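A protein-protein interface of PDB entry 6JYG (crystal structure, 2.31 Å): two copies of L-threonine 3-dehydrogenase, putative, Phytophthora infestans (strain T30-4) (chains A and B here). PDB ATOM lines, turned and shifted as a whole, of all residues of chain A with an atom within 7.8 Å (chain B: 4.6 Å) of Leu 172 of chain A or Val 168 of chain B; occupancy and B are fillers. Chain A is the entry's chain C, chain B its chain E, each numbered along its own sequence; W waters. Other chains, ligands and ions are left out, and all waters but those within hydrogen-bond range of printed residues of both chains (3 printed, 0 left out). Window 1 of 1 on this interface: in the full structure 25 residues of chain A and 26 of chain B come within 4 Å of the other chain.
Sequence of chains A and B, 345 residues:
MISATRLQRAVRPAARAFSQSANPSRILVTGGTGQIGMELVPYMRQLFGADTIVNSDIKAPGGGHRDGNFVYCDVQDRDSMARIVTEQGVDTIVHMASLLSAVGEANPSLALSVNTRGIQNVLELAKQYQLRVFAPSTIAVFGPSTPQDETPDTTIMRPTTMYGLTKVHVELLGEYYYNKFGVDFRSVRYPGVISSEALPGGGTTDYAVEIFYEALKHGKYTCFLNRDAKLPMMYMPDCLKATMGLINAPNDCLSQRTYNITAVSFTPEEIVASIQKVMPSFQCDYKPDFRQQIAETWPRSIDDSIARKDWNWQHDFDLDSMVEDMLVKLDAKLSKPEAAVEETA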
ATOM      1  N   ILE A 119      29.307  -3.120   7.245  1.00  0.00           N
ATOM      2  CA  ILE A 119      28.834  -3.633   5.976  1.00  0.00           C
ATOM      3  C   ILE A 119      27.547  -2.878   5.573  1.00  0.00           C
ATOM      4  O   ILE A 119      27.258  -2.756   4.428  1.00  0.00           O
ATOM      5  CB  ILE A 119      28.612  -5.213   5.939  1.00  0.00           C
ATOM      6  CG1 ILE A 119      28.394  -5.718   4.502  1.00  0.00           C
ATOM      7  CG2 ILE A 119      27.419  -5.702   6.840  1.00  0.00           C
ATOM      8  CD1 ILE A 119      29.553  -5.529   3.550  1.00  0.00           C
ATOM      9  N   LEU A 123      27.359  -0.779   2.058  1.00  0.00           N
ATOM     10  CA  LEU A 123      26.465  -1.279   0.998  1.00  0.00           C
ATOM     11  C   LEU A 123      25.519  -0.123   0.507  1.00  0.00           C
ATOM     12  O   LEU A 123      25.289   0.071  -0.713  1.00  0.00           O
ATOM     13  CB  LEU A 123      25.720  -2.584   1.411  1.00  0.00           C
ATOM     14  CG  LEU A 123      26.576  -3.885   1.268  1.00  0.00           C
ATOM     15  CD1 LEU A 123      25.812  -5.078   1.668  1.00  0.00           C
ATOM     16  CD2 LEU A 123      27.120  -4.114  -0.137  1.00  0.00           C
ATOM     17  N   SER A 137      34.275 -12.872   4.009  1.00  0.00           N
ATOM     18  CA  SER A 137      33.573 -13.666   5.000  1.00  0.00           C
ATOM     19  C   SER A 137      34.623 -14.591   5.689  1.00  0.00           C
ATOM     20  O   SER A 137      35.829 -14.467   5.514  1.00  0.00           O
ATOM     21  CB  SER A 137      32.343 -14.431   4.408  1.00  0.00           C
ATOM     22  OG  SER A 137      31.552 -15.047   5.499  1.00  0.00           O
ATOM     23  N   MET A 157      24.320 -22.899   8.249  1.00  0.00           N
ATOM     24  CA  MET A 157      25.198 -21.937   8.892  1.00  0.00           C
ATOM     25  C   MET A 157      24.581 -21.476  10.202  1.00  0.00           C
ATOM     26  O   MET A 157      23.782 -20.581  10.229  1.00  0.00           O
ATOM     27  CB  MET A 157      25.526 -20.769   7.946  1.00  0.00           C
ATOM     28  CG  MET A 157      26.447 -21.076   6.692  1.00  0.00           C
ATOM     29  SD  MET A 157      26.551 -19.642   5.520  1.00  0.00           S
ATOM     30  CE  MET A 157      27.679 -20.119   4.201  1.00  0.00           C
ATOM     31  N   ARG A 158      24.952 -22.130  11.297  1.00  0.00           N
ATOM     32  CA  ARG A 158      24.487 -21.701  12.638  1.00  0.00           C
ATOM     33  C   ARG A 158      25.723 -21.421  13.474  1.00  0.00           C
ATOM     34  O   ARG A 158      26.185 -22.245  14.160  1.00  0.00           O
ATOM     35  CB  ARG A 158      23.542 -22.719  13.260  1.00  0.00           C
ATOM     36  CG  ARG A 158      22.398 -23.082  12.284  1.00  0.00           C
ATOM     37  CD  ARG A 158      21.522 -21.874  12.036  1.00  0.00           C
ATOM     38  NE  ARG A 158      20.631 -21.782  13.220  1.00  0.00           N
ATOM     39  CZ  ARG A 158      19.440 -21.181  13.219  1.00  0.00           C
ATOM     40  NH1 ARG A 158      18.919 -20.561  12.086  1.00  0.00           N
ATOM     41  NH2 ARG A 158      18.786 -21.191  14.371  1.00  0.00           N
ATOM     42  N   LEU A 165      28.183 -14.881  13.448  1.00  0.00           N
ATOM     43  CA  LEU A 165      26.832 -14.511  13.073  1.00  0.00           C
ATOM     44  C   LEU A 165      26.931 -13.129  12.320  1.00  0.00           C
ATOM     45  O   LEU A 165      26.192 -12.869  11.352  1.00  0.00           O
ATOM     46  CB  LEU A 165      25.814 -14.551  14.275  1.00  0.00           C
ATOM     47  CG  LEU A 165      25.961 -13.465  15.367  1.00  0.00           C
ATOM     48  CD1 LEU A 165      25.192 -12.212  14.985  1.00  0.00           C
ATOM     49  CD2 LEU A 165      25.563 -14.005  16.749  1.00  0.00           C
ATOM     50  N   THR A 166      27.813 -12.224  12.762  1.00  0.00           N
ATOM     51  CA  THR A 166      27.911 -10.955  11.999  1.00  0.00           C
ATOM     52  C   THR A 166      28.326 -11.157  10.527  1.00  0.00           C
ATOM     53  O   THR A 166      27.870 -10.432   9.663  1.00  0.00           O
ATOM     54  CB  THR A 166      28.832  -9.930  12.630  1.00  0.00           C
ATOM     55  OG1 THR A 166      30.143 -10.347  12.407  1.00  0.00           O
ATOM     56  CG2 THR A 166      28.635  -9.897  13.991  1.00  0.00           C
ATOM     57  N   LYS A 167      29.157 -12.122  10.262  1.00  0.00           N
ATOM     58  CA  LYS A 167      29.565 -12.404   8.891  1.00  0.00           C
ATOM     59  C   LYS A 167      28.505 -13.078   7.978  1.00  0.00           C
ATOM     60  O   LYS A 167      28.635 -13.008   6.777  1.00  0.00           O
ATOM     61  CB  LYS A 167      30.845 -13.211   8.903  1.00  0.00           C
ATOM     62  CG  LYS A 167      32.058 -12.449   9.490  1.00  0.00           C
ATOM     63  CD  LYS A 167      32.593 -11.614   8.312  1.00  0.00           C
ATOM     64  CE  LYS A 167      33.831 -10.806   8.654  1.00  0.00           C
ATOM     65  NZ  LYS A 167      33.863  -9.717   7.664  1.00  0.00           N
ATOM     66  N   VAL A 168      27.440 -13.668   8.543  1.00  0.00           N
ATOM     67  CA  VAL A 168      26.386 -14.282   7.803  1.00  0.00           C
ATOM     68  C   VAL A 168      25.538 -13.124   7.388  1.00  0.00           C
ATOM     69  O   VAL A 168      25.085 -13.004   6.227  1.00  0.00           O
ATOM     70  CB  VAL A 168      25.561 -15.177   8.744  1.00  0.00           C
ATOM     71  CG1 VAL A 168      24.245 -15.673   8.091  1.00  0.00           C
ATOM     72  CG2 VAL A 168      26.386 -16.425   9.069  1.00  0.00           C
ATOM     73  N   HIS A 169      25.346 -12.192   8.337  1.00  0.00           N
ATOM     74  CA  HIS A 169      24.677 -10.971   7.934  1.00  0.00           C
ATOM     75  C   HIS A 169      25.535 -10.237   6.863  1.00  0.00           C
ATOM     76  O   HIS A 169      25.006  -9.852   5.777  1.00  0.00           O
ATOM     77  CB  HIS A 169      24.409 -10.171   9.128  1.00  0.00           C
ATOM     78  CG  HIS A 169      23.777  -8.839   8.847  1.00  0.00           C
ATOM     79  ND1 HIS A 169      22.458  -8.698   8.466  1.00  0.00           N
ATOM     80  CD2 HIS A 169      24.291  -7.589   8.928  1.00  0.00           C
ATOM     81  CE1 HIS A 169      22.189  -7.416   8.335  1.00  0.00           C
ATOM     82  NE2 HIS A 169      23.271  -6.726   8.652  1.00  0.00           N
ATOM     83  N   VAL A 170      26.856 -10.139   7.079  1.00  0.00           N
ATOM     84  CA  VAL A 170      27.650  -9.623   5.918  1.00  0.00           C
ATOM     85  C   VAL A 170      27.287 -10.264   4.503  1.00  0.00           C
ATOM     86  O   VAL A 170      26.882  -9.537   3.557  1.00  0.00           O
ATOM     87  CB  VAL A 170      29.083  -9.733   6.226  1.00  0.00           C
ATOM     88  CG1 VAL A 170      29.810  -9.558   4.947  1.00  0.00           C
ATOM     89  CG2 VAL A 170      29.481  -8.676   7.291  1.00  0.00           C
ATOM     90  N   GLU A 171      27.361 -11.618   4.401  1.00  0.00           N
ATOM     91  CA  GLU A 171      27.045 -12.338   3.144  1.00  0.00           C
ATOM     92  C   GLU A 171      25.628 -12.136   2.631  1.00  0.00           C
ATOM     93  O   GLU A 171      25.406 -11.980   1.430  1.00  0.00           O
ATOM     94  CB  GLU A 171      27.238 -13.880   3.310  1.00  0.00           C
ATOM     95  CG  GLU A 171      28.667 -14.313   3.469  1.00  0.00           C
ATOM     96  CD  GLU A 171      28.769 -15.819   3.630  1.00  0.00           C
ATOM     97  OE1 GLU A 171      27.963 -16.506   2.933  1.00  0.00           O
ATOM     98  OE2 GLU A 171      29.653 -16.306   4.409  1.00  0.00           O
ATOM     99  N   LEU A 172      24.667 -12.264   3.553  1.00  0.00           N
ATOM    100  CA  LEU A 172      23.310 -12.229   3.193  1.00  0.00           C
ATOM    101  C   LEU A 172      22.907 -10.860   2.688  1.00  0.00           C
ATOM    102  O   LEU A 172      22.086 -10.785   1.730  1.00  0.00           O
ATOM    103  CB  LEU A 172      22.367 -12.572   4.395  1.00  0.00           C
ATOM    104  CG  LEU A 172      22.351 -14.032   4.896  1.00  0.00           C
ATOM    105  CD1 LEU A 172      21.110 -14.361   5.841  1.00  0.00           C
ATOM    106  CD2 LEU A 172      22.550 -15.055   3.726  1.00  0.00           C
ATOM    107  N   LEU A 173      23.360  -9.802   3.394  1.00  0.00           N
ATOM    108  CA  LEU A 173      23.105  -8.454   3.002  1.00  0.00           C
ATOM    109  C   LEU A 173      23.832  -8.116   1.618  1.00  0.00           C
ATOM    110  O   LEU A 173      23.235  -7.392   0.731  1.00  0.00           O
ATOM    111  CB  LEU A 173      23.532  -7.449   4.118  1.00  0.00           C
ATOM    112  CG  LEU A 173      23.013  -6.046   3.984  1.00  0.00           C
ATOM    113  CD1 LEU A 173      21.529  -6.128   4.072  1.00  0.00           C
ATOM    114  CD2 LEU A 173      23.537  -5.048   5.089  1.00  0.00           C
ATOM    115  N   GLY A 174      25.091  -8.563   1.465  1.00  0.00           N
ATOM    116  CA  GLY A 174      25.876  -8.185   0.244  1.00  0.00           C
ATOM    117  C   GLY A 174      25.076  -8.859  -0.913  1.00  0.00           C
ATOM    118  O   GLY A 174      24.827  -8.235  -1.999  1.00  0.00           O
ATOM    119  N   GLU A 175      24.616 -10.127  -0.701  1.00  0.00           N
ATOM    120  CA  GLU A 175      23.848 -10.775  -1.802  1.00  0.00           C
ATOM    121  C   GLU A 175      22.577 -10.038  -2.160  1.00  0.00           C
ATOM    122  O   GLU A 175      22.223  -9.933  -3.356  1.00  0.00           O
ATOM    123  CB  GLU A 175      23.442 -12.222  -1.522  1.00  0.00           C
ATOM    124  CG  GLU A 175      24.175 -13.245  -2.350  1.00  0.00           C
ATOM    125  CD  GLU A 175      24.653 -14.427  -1.491  1.00  0.00           C
ATOM    126  OE1 GLU A 175      25.860 -14.452  -1.037  1.00  0.00           O
ATOM    127  OE2 GLU A 175      23.786 -15.311  -1.277  1.00  0.00           O
ATOM    128  N   TYR A 176      21.896  -9.573  -1.119  1.00  0.00           N
ATOM    129  CA  TYR A 176      20.699  -8.840  -1.330  1.00  0.00           C
ATOM    130  C   TYR A 176      20.923  -7.540  -2.162  1.00  0.00           C
ATOM    131  O   TYR A 176      20.234  -7.357  -3.168  1.00  0.00           O
ATOM    132  CB  TYR A 176      20.045  -8.483   0.005  1.00  0.00           C
ATOM    133  CG  TYR A 176      18.773  -7.651  -0.207  1.00  0.00           C
ATOM    134  CD1 TYR A 176      17.527  -8.287  -0.465  1.00  0.00           C
ATOM    135  CD2 TYR A 176      18.839  -6.297  -0.145  1.00  0.00           C
ATOM    136  CE1 TYR A 176      16.398  -7.566  -0.709  1.00  0.00           C
ATOM    137  CE2 TYR A 176      17.712  -5.531  -0.297  1.00  0.00           C
ATOM    138  CZ  TYR A 176      16.490  -6.154  -0.583  1.00  0.00           C
ATOM    139  OH  TYR A 176      15.378  -5.354  -0.713  1.00  0.00           O
ATOM    140  N   TYR A 177      21.867  -6.703  -1.766  1.00  0.00           N
ATOM    141  CA  TYR A 177      22.278  -5.581  -2.549  1.00  0.00           C
ATOM    142  C   TYR A 177      22.632  -5.814  -4.036  1.00  0.00           C
ATOM    143  O   TYR A 177      22.231  -4.961  -4.904  1.00  0.00           O
ATOM    144  CB  TYR A 177      23.461  -4.812  -1.904  1.00  0.00           C
ATOM    145  CG  TYR A 177      22.925  -3.854  -0.904  1.00  0.00           C
ATOM    146  CD1 TYR A 177      22.400  -4.322   0.306  1.00  0.00           C
ATOM    147  CD2 TYR A 177      22.868  -2.498  -1.205  1.00  0.00           C
ATOM    148  CE1 TYR A 177      21.849  -3.449   1.223  1.00  0.00           C
ATOM    149  CE2 TYR A 177      22.371  -1.601  -0.314  1.00  0.00           C
ATOM    150  CZ  TYR A 177      21.866  -2.068   0.878  1.00  0.00           C
ATOM    151  OH  TYR A 177      21.443  -1.155   1.779  1.00  0.00           O
ATOM    152  N   TYR A 178      23.360  -6.920  -4.304  1.00  0.00           N
ATOM    153  CA  TYR A 178      23.534  -7.439  -5.663  1.00  0.00           C
ATOM    154  C   TYR A 178      22.198  -7.692  -6.421  1.00  0.00           C
ATOM    155  O   TYR A 178      21.976  -7.125  -7.510  1.00  0.00           O
ATOM    156  CB  TYR A 178      24.340  -8.719  -5.671  1.00  0.00           C
ATOM    157  CG  TYR A 178      24.576  -9.171  -7.082  1.00  0.00           C
ATOM    158  CD1 TYR A 178      25.582  -8.548  -7.850  1.00  0.00           C
ATOM    159  CD2 TYR A 178      23.862 -10.288  -7.644  1.00  0.00           C
ATOM    160  CE1 TYR A 178      25.840  -8.975  -9.161  1.00  0.00           C
ATOM    161  CE2 TYR A 178      24.104 -10.719  -8.980  1.00  0.00           C
ATOM    162  CZ  TYR A 178      25.107 -10.042  -9.716  1.00  0.00           C
ATOM    163  OH  TYR A 178      25.404 -10.323 -11.010  1.00  0.00           O
ATOM    164  N   ASN A 179      21.320  -8.525  -5.843  1.00  0.00           N
ATOM    165  CA  ASN A 179      20.132  -8.950  -6.583  1.00  0.00           C
ATOM    166  C   ASN A 179      19.134  -7.842  -6.643  1.00  0.00           C
ATOM    167  O   ASN A 179      18.355  -7.772  -7.579  1.00  0.00           O
ATOM    168  CB  ASN A 179      19.512 -10.175  -5.968  1.00  0.00           C
ATOM    169  CG  ASN A 179      20.353 -11.436  -6.256  1.00  0.00           C
ATOM    170  OD1 ASN A 179      20.600 -11.769  -7.421  1.00  0.00           O
ATOM    171  ND2 ASN A 179      20.805 -12.114  -5.219  1.00  0.00           N
ATOM    172  N   PHE A 185      28.847  -6.970  -5.543  1.00  0.00           N
ATOM    173  CA  PHE A 185      29.257  -7.409  -4.258  1.00  0.00           C
ATOM    174  C   PHE A 185      29.916  -8.792  -4.389  1.00  0.00           C
ATOM    175  O   PHE A 185      29.427  -9.658  -5.080  1.00  0.00           O
ATOM    176  CB  PHE A 185      28.045  -7.634  -3.331  1.00  0.00           C
ATOM    177  CG  PHE A 185      28.460  -8.182  -2.011  1.00  0.00           C
ATOM    178  CD1 PHE A 185      28.344  -9.555  -1.736  1.00  0.00           C
ATOM    179  CD2 PHE A 185      29.123  -7.344  -1.070  1.00  0.00           C
ATOM    180  CE1 PHE A 185      28.769 -10.043  -0.474  1.00  0.00           C
ATOM    181  CE2 PHE A 185      29.636  -7.840   0.173  1.00  0.00           C
ATOM    182  CZ  PHE A 185      29.401  -9.174   0.491  1.00  0.00           C
ATOM    183  N   SER A 187      32.454 -11.594  -1.877  1.00  0.00           N
ATOM    184  CA  SER A 187      33.307 -12.078  -0.802  1.00  0.00           C
ATOM    185  C   SER A 187      33.948 -13.468  -1.096  1.00  0.00           C
ATOM    186  O   SER A 187      33.427 -14.359  -1.882  1.00  0.00           O
ATOM    187  CB  SER A 187      32.528 -12.285   0.544  1.00  0.00           C
ATOM    188  OG  SER A 187      31.223 -12.116   0.111  1.00  0.00           O
ATOM    189  N   THR A 258      29.520 -15.011  -2.703  1.00  0.00           N
ATOM    190  CA  THR A 258      30.528 -15.492  -1.759  1.00  0.00           C
ATOM    191  C   THR A 258      31.196 -16.828  -2.134  1.00  0.00           C
ATOM    192  O   THR A 258      30.524 -17.738  -2.575  1.00  0.00           O
ATOM    193  CB  THR A 258      29.864 -15.616  -0.417  1.00  0.00           C
ATOM    194  OG1 THR A 258      29.052 -14.463  -0.305  1.00  0.00           O
ATOM    195  CG2 THR A 258      30.946 -15.660   0.758  1.00  0.00           C
ATOM    196  N   VAL B 141      12.995 -16.860   6.109  1.00  0.00           N
ATOM    197  CA  VAL B 141      14.454 -17.108   6.331  1.00  0.00           C
ATOM    198  C   VAL B 141      15.016 -18.093   5.294  1.00  0.00           C
ATOM    199  O   VAL B 141      16.212 -18.226   5.115  1.00  0.00           O
ATOM    200  CB  VAL B 141      14.726 -17.617   7.793  1.00  0.00           C
ATOM    201  CG1 VAL B 141      14.406 -16.542   8.845  1.00  0.00           C
ATOM    202  CG2 VAL B 141      13.836 -18.783   8.096  1.00  0.00           C
ATOM    203  N   MET B 157      19.721 -21.566   4.494  1.00  0.00           N
ATOM    204  CA  MET B 157      18.933 -20.370   4.737  1.00  0.00           C
ATOM    205  C   MET B 157      19.539 -19.155   3.962  1.00  0.00           C
ATOM    206  O   MET B 157      20.296 -18.403   4.501  1.00  0.00           O
ATOM    207  CB  MET B 157      18.836 -20.194   6.220  1.00  0.00           C
ATOM    208  CG  MET B 157      17.712 -21.021   6.853  1.00  0.00           C
ATOM    209  SD  MET B 157      17.519 -20.449   8.554  1.00  0.00           S
ATOM    210  CE  MET B 157      16.585 -21.681   9.441  1.00  0.00           C
ATOM    211  N   ARG B 158      19.192 -18.988   2.683  1.00  0.00           N
ATOM    212  CA  ARG B 158      19.779 -17.881   1.877  1.00  0.00           C
ATOM    213  C   ARG B 158      18.620 -17.040   1.391  1.00  0.00           C
ATOM    214  O   ARG B 158      18.228 -17.128   0.232  1.00  0.00           O
ATOM    215  CB  ARG B 158      20.512 -18.479   0.698  1.00  0.00           C
ATOM    216  CG  ARG B 158      21.818 -19.213   1.048  1.00  0.00           C
ATOM    217  CD  ARG B 158      23.055 -18.436   0.537  1.00  0.00           C
ATOM    218  NE  ARG B 158      23.713 -18.100   1.784  1.00  0.00           N
ATOM    219  CZ  ARG B 158      24.851 -17.426   1.925  1.00  0.00           C
ATOM    220  NH1 ARG B 158      25.491 -16.914   0.864  1.00  0.00           N
ATOM    221  NH2 ARG B 158      25.312 -17.258   3.161  1.00  0.00           N
ATOM    222  N   PRO B 159      17.975 -16.284   2.271  1.00  0.00           N
ATOM    223  CA  PRO B 159      16.709 -15.704   1.743  1.00  0.00           C
ATOM    224  C   PRO B 159      16.950 -14.522   0.798  1.00  0.00           C
ATOM    225  O   PRO B 159      18.039 -13.885   0.849  1.00  0.00           O
ATOM    226  CB  PRO B 159      15.979 -15.273   3.005  1.00  0.00           C
ATOM    227  CG  PRO B 159      17.121 -15.053   3.993  1.00  0.00           C
ATOM    228  CD  PRO B 159      18.143 -16.071   3.700  1.00  0.00           C
ATOM    229  N   GLY B 164      13.434 -11.395   5.114  1.00  0.00           N
ATOM    230  CA  GLY B 164      13.999 -12.681   5.592  1.00  0.00           C
ATOM    231  C   GLY B 164      15.476 -12.653   6.108  1.00  0.00           C
ATOM    232  O   GLY B 164      15.861 -13.390   7.081  1.00  0.00           O
ATOM    233  N   LEU B 165      16.308 -11.826   5.471  1.00  0.00           N
ATOM    234  CA  LEU B 165      17.679 -11.838   5.860  1.00  0.00           C
ATOM    235  C   LEU B 165      17.694 -11.163   7.268  1.00  0.00           C
ATOM    236  O   LEU B 165      18.489 -11.541   8.141  1.00  0.00           O
ATOM    237  CB  LEU B 165      18.583 -11.184   4.789  1.00  0.00           C
ATOM    238  CG  LEU B 165      18.562  -9.654   4.707  1.00  0.00           C
ATOM    239  CD1 LEU B 165      19.585  -9.066   5.663  1.00  0.00           C
ATOM    240  CD2 LEU B 165      18.774  -9.275   3.254  1.00  0.00           C
ATOM    241  N   THR B 166      16.824 -10.192   7.540  1.00  0.00           N
ATOM    242  CA  THR B 166      16.848  -9.621   8.923  1.00  0.00           C
ATOM    243  C   THR B 166      16.446 -10.628   9.929  1.00  0.00           C
ATOM    244  O   THR B 166      16.931 -10.572  11.094  1.00  0.00           O
ATOM    245  CB  THR B 166      15.992  -8.384   9.121  1.00  0.00           C
ATOM    246  OG1 THR B 166      14.595  -8.722   8.955  1.00  0.00           O
ATOM    247  CG2 THR B 166      16.394  -7.429   8.132  1.00  0.00           C
ATOM    248  N   LYS B 167      15.572 -11.571   9.534  1.00  0.00           N
ATOM    249  CA  LYS B 167      15.110 -12.601  10.535  1.00  0.00           C
ATOM    250  C   LYS B 167      16.081 -13.756  10.787  1.00  0.00           C
ATOM    251  O   LYS B 167      15.976 -14.419  11.827  1.00  0.00           O
ATOM    252  CB  LYS B 167      13.703 -13.086  10.214  1.00  0.00           C
ATOM    253  CG  LYS B 167      12.667 -11.951  10.311  1.00  0.00           C
ATOM    254  CD  LYS B 167      12.233 -11.673  11.744  1.00  0.00           C
ATOM    255  CE  LYS B 167      10.768 -11.328  11.765  1.00  0.00           C
ATOM    256  NZ  LYS B 167      10.258 -11.067  13.161  1.00  0.00           N
ATOM    257  N   VAL B 168      17.047 -14.023   9.875  1.00  0.00           N
ATOM    258  CA  VAL B 168      18.028 -14.986  10.207  1.00  0.00           C
ATOM    259  C   VAL B 168      18.908 -14.292  11.205  1.00  0.00           C
ATOM    260  O   VAL B 168      19.425 -14.905  12.159  1.00  0.00           O
ATOM    261  CB  VAL B 168      18.810 -15.624   9.049  1.00  0.00           C
ATOM    262  CG1 VAL B 168      17.859 -16.114   7.984  1.00  0.00           C
ATOM    263  CG2 VAL B 168      19.672 -14.657   8.416  1.00  0.00           C
ATOM    264  N   HIS B 169      19.016 -12.986  11.081  1.00  0.00           N
ATOM    265  CA  HIS B 169      19.818 -12.242  12.074  1.00  0.00           C
ATOM    266  C   HIS B 169      19.113 -12.344  13.459  1.00  0.00           C
ATOM    267  O   HIS B 169      19.713 -12.637  14.483  1.00  0.00           O
ATOM    268  CB  HIS B 169      20.112 -10.803  11.603  1.00  0.00           C
ATOM    269  CG  HIS B 169      20.862 -10.004  12.613  1.00  0.00           C
ATOM    270  ND1 HIS B 169      22.167 -10.305  12.987  1.00  0.00           N
ATOM    271  CD2 HIS B 169      20.489  -8.943  13.350  1.00  0.00           C
ATOM    272  CE1 HIS B 169      22.557  -9.477  13.941  1.00  0.00           C
ATOM    273  NE2 HIS B 169      21.572  -8.619  14.154  1.00  0.00           N
ATOM    274  N   VAL B 170      17.798 -12.175  13.446  1.00  0.00           N
ATOM    275  CA  VAL B 170      17.046 -12.463  14.670  1.00  0.00           C
ATOM    276  C   VAL B 170      17.414 -13.812  15.396  1.00  0.00           C
ATOM    277  O   VAL B 170      17.745 -13.826  16.602  1.00  0.00           O
ATOM    278  CB  VAL B 170      15.555 -12.362  14.397  1.00  0.00           C
ATOM    279  CG1 VAL B 170      14.739 -12.961  15.552  1.00  0.00           C
ATOM    280  CG2 VAL B 170      15.257 -10.889  14.124  1.00  0.00           C
ATOM    281  N   GLU B 171      17.396 -14.910  14.623  1.00  0.00           N
ATOM    282  CA  GLU B 171      17.564 -16.279  15.175  1.00  0.00           C
ATOM    283  C   GLU B 171      18.923 -16.477  15.707  1.00  0.00           C
ATOM    284  O   GLU B 171      19.098 -17.002  16.787  1.00  0.00           O
ATOM    285  CB  GLU B 171      17.322 -17.355  14.100  1.00  0.00           C
ATOM    286  CG  GLU B 171      15.922 -17.319  13.439  1.00  0.00           C
ATOM    287  CD  GLU B 171      15.686 -18.503  12.516  1.00  0.00           C
ATOM    288  OE1 GLU B 171      16.553 -19.424  12.529  1.00  0.00           O
ATOM    289  OE2 GLU B 171      14.639 -18.542  11.810  1.00  0.00           O
ATOM    290  N   LEU B 172      19.897 -16.097  14.886  1.00  0.00           N
ATOM    291  CA  LEU B 172      21.292 -16.296  15.172  1.00  0.00           C
ATOM    292  C   LEU B 172      21.661 -15.458  16.370  1.00  0.00           C
ATOM    293  O   LEU B 172      22.487 -15.903  17.148  1.00  0.00           O
ATOM    294  CB  LEU B 172      22.223 -15.779  13.996  1.00  0.00           C
ATOM    295  CG  LEU B 172      22.189 -16.641  12.712  1.00  0.00           C
ATOM    296  CD1 LEU B 172      23.331 -16.454  11.575  1.00  0.00           C
ATOM    297  CD2 LEU B 172      21.936 -18.136  13.029  1.00  0.00           C
HETATM  298  O   HOH W   1      20.768 -20.031   9.543  1.00  0.00           O
HETATM  299  O   HOH W   2      23.282 -12.532  11.813  1.00  0.00           O
HETATM  300  O   HOH W   3      20.551 -12.259   0.513  1.00  0.00           O
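NH2 of Arg 158 of chain B lies within hydrogen-bond range of SD of Met 157 of chain A (3.6 Å).
NH1 of Arg 158 of chain A lies within salt-bridge range of OE1 of Glu 171 of chain B, 2.7 Å away.
The side-chain carboxylate (OE1) of Glu 171 of chain A is in salt-bridge range of the guanidinium group (NH2) of Arg 158 of chain B.
The guanidinium group of Arg 158 of chain B lies within salt-bridge range of the side-chain carboxylate of Glu 175 of chain A, 3.1 Å away.
The side-chain amide nitrogen (ND2) of Asn 179 of chain A sits at hydrogen-bond distance from the backbone carbonyl oxygen (O) of Glu 175 of chain A (3.2 Å).
OG1 of Thr 258 of chain A lies within hydrogen-bond range of OE1 of Glu 175 of chain A (3.3 Å).
Among the printed residues, merely in contact across the chains: Leu 172 of chain A with Val 168 of chain B (3.0 Å), Tyr 176 of chain A with Leu 165 of chain B (3.6 Å), Leu 172 of chain A with Arg 158 of chain B (3.6 Å), Leu 165 of chain A with Leu 172 of chain B (3.6 Å), Val 168 of chain A with Leu 172 of chain B (3.7 Å), Arg 158 of chain A with Met 157 of chain B (3.7 Å), Leu 173 of chain A with Leu 165 of chain B (3.9 Å), Arg 158 of chain A with Leu 172 of chain B (3.9 Å), Leu 165 of chain A with His 169 of chain B (3.9 Å) and Leu 172 of chain A with Leu 165 of chain B (3.9 Å).
Leu 172 of chain A touches three residues of chain B.
Of the printed residues of chain A, Leu 165 of chain B touches Leu 172 (3.9 Å), Leu 173 (3.9 Å) and Tyr 176 (3.6 Å).
Of chain A, only Leu 172 comes within 4 Å of Val 168 of chain B.
Printed residues of chain A within 4 Å of Glu 171 of chain B: Arg 158.
The nearest residue of chain B that does not touch Leu 172 of chain A is Pro 159 of chain B (4.04 Å).
The nearest residue of chain A that does not touch Val 168 of chain B is Val 168 of chain A (4.7 Å).
The nearest printed residue of chain A that does not touch His 169 of chain B is His 169 of chain A (4.4 Å).
Printed residues of chain A that touch a printed residue of chain B: Met 157, Arg 158, Leu 165, Val 168, Glu 171, Leu 172, Leu 173, Glu 175 and Tyr 176.
Hydrophobic or aromatic side chains of chain A within 4 Å of the printed part of chain B: Met 157, Leu 165, Val 168, Leu 172, Leu 173 and Tyr 176.
Along chain B the printed residues that touch a printed residue of chain A span positions 157 to 172.
Among the printed residues, 14 pairs touch across the chains.
Arg 158 of chain A touches Glu 171 of chain B, and with the chains exchanged Glu 171 of chain A touches Arg 158 of chain B.
Leu 165 of chain A touches His 169 of chain B, but with the chains exchanged His 169 of chain A does not touch Leu 165 of chain B (4.03 Å).
Water W2 lies within hydrogen-bond range of a ring nitrogen (ND1) of His 169 of chain B (2.8 Å) and the backbone carbonyl oxygen (O) of Leu 165 of chain A (3.0 Å).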
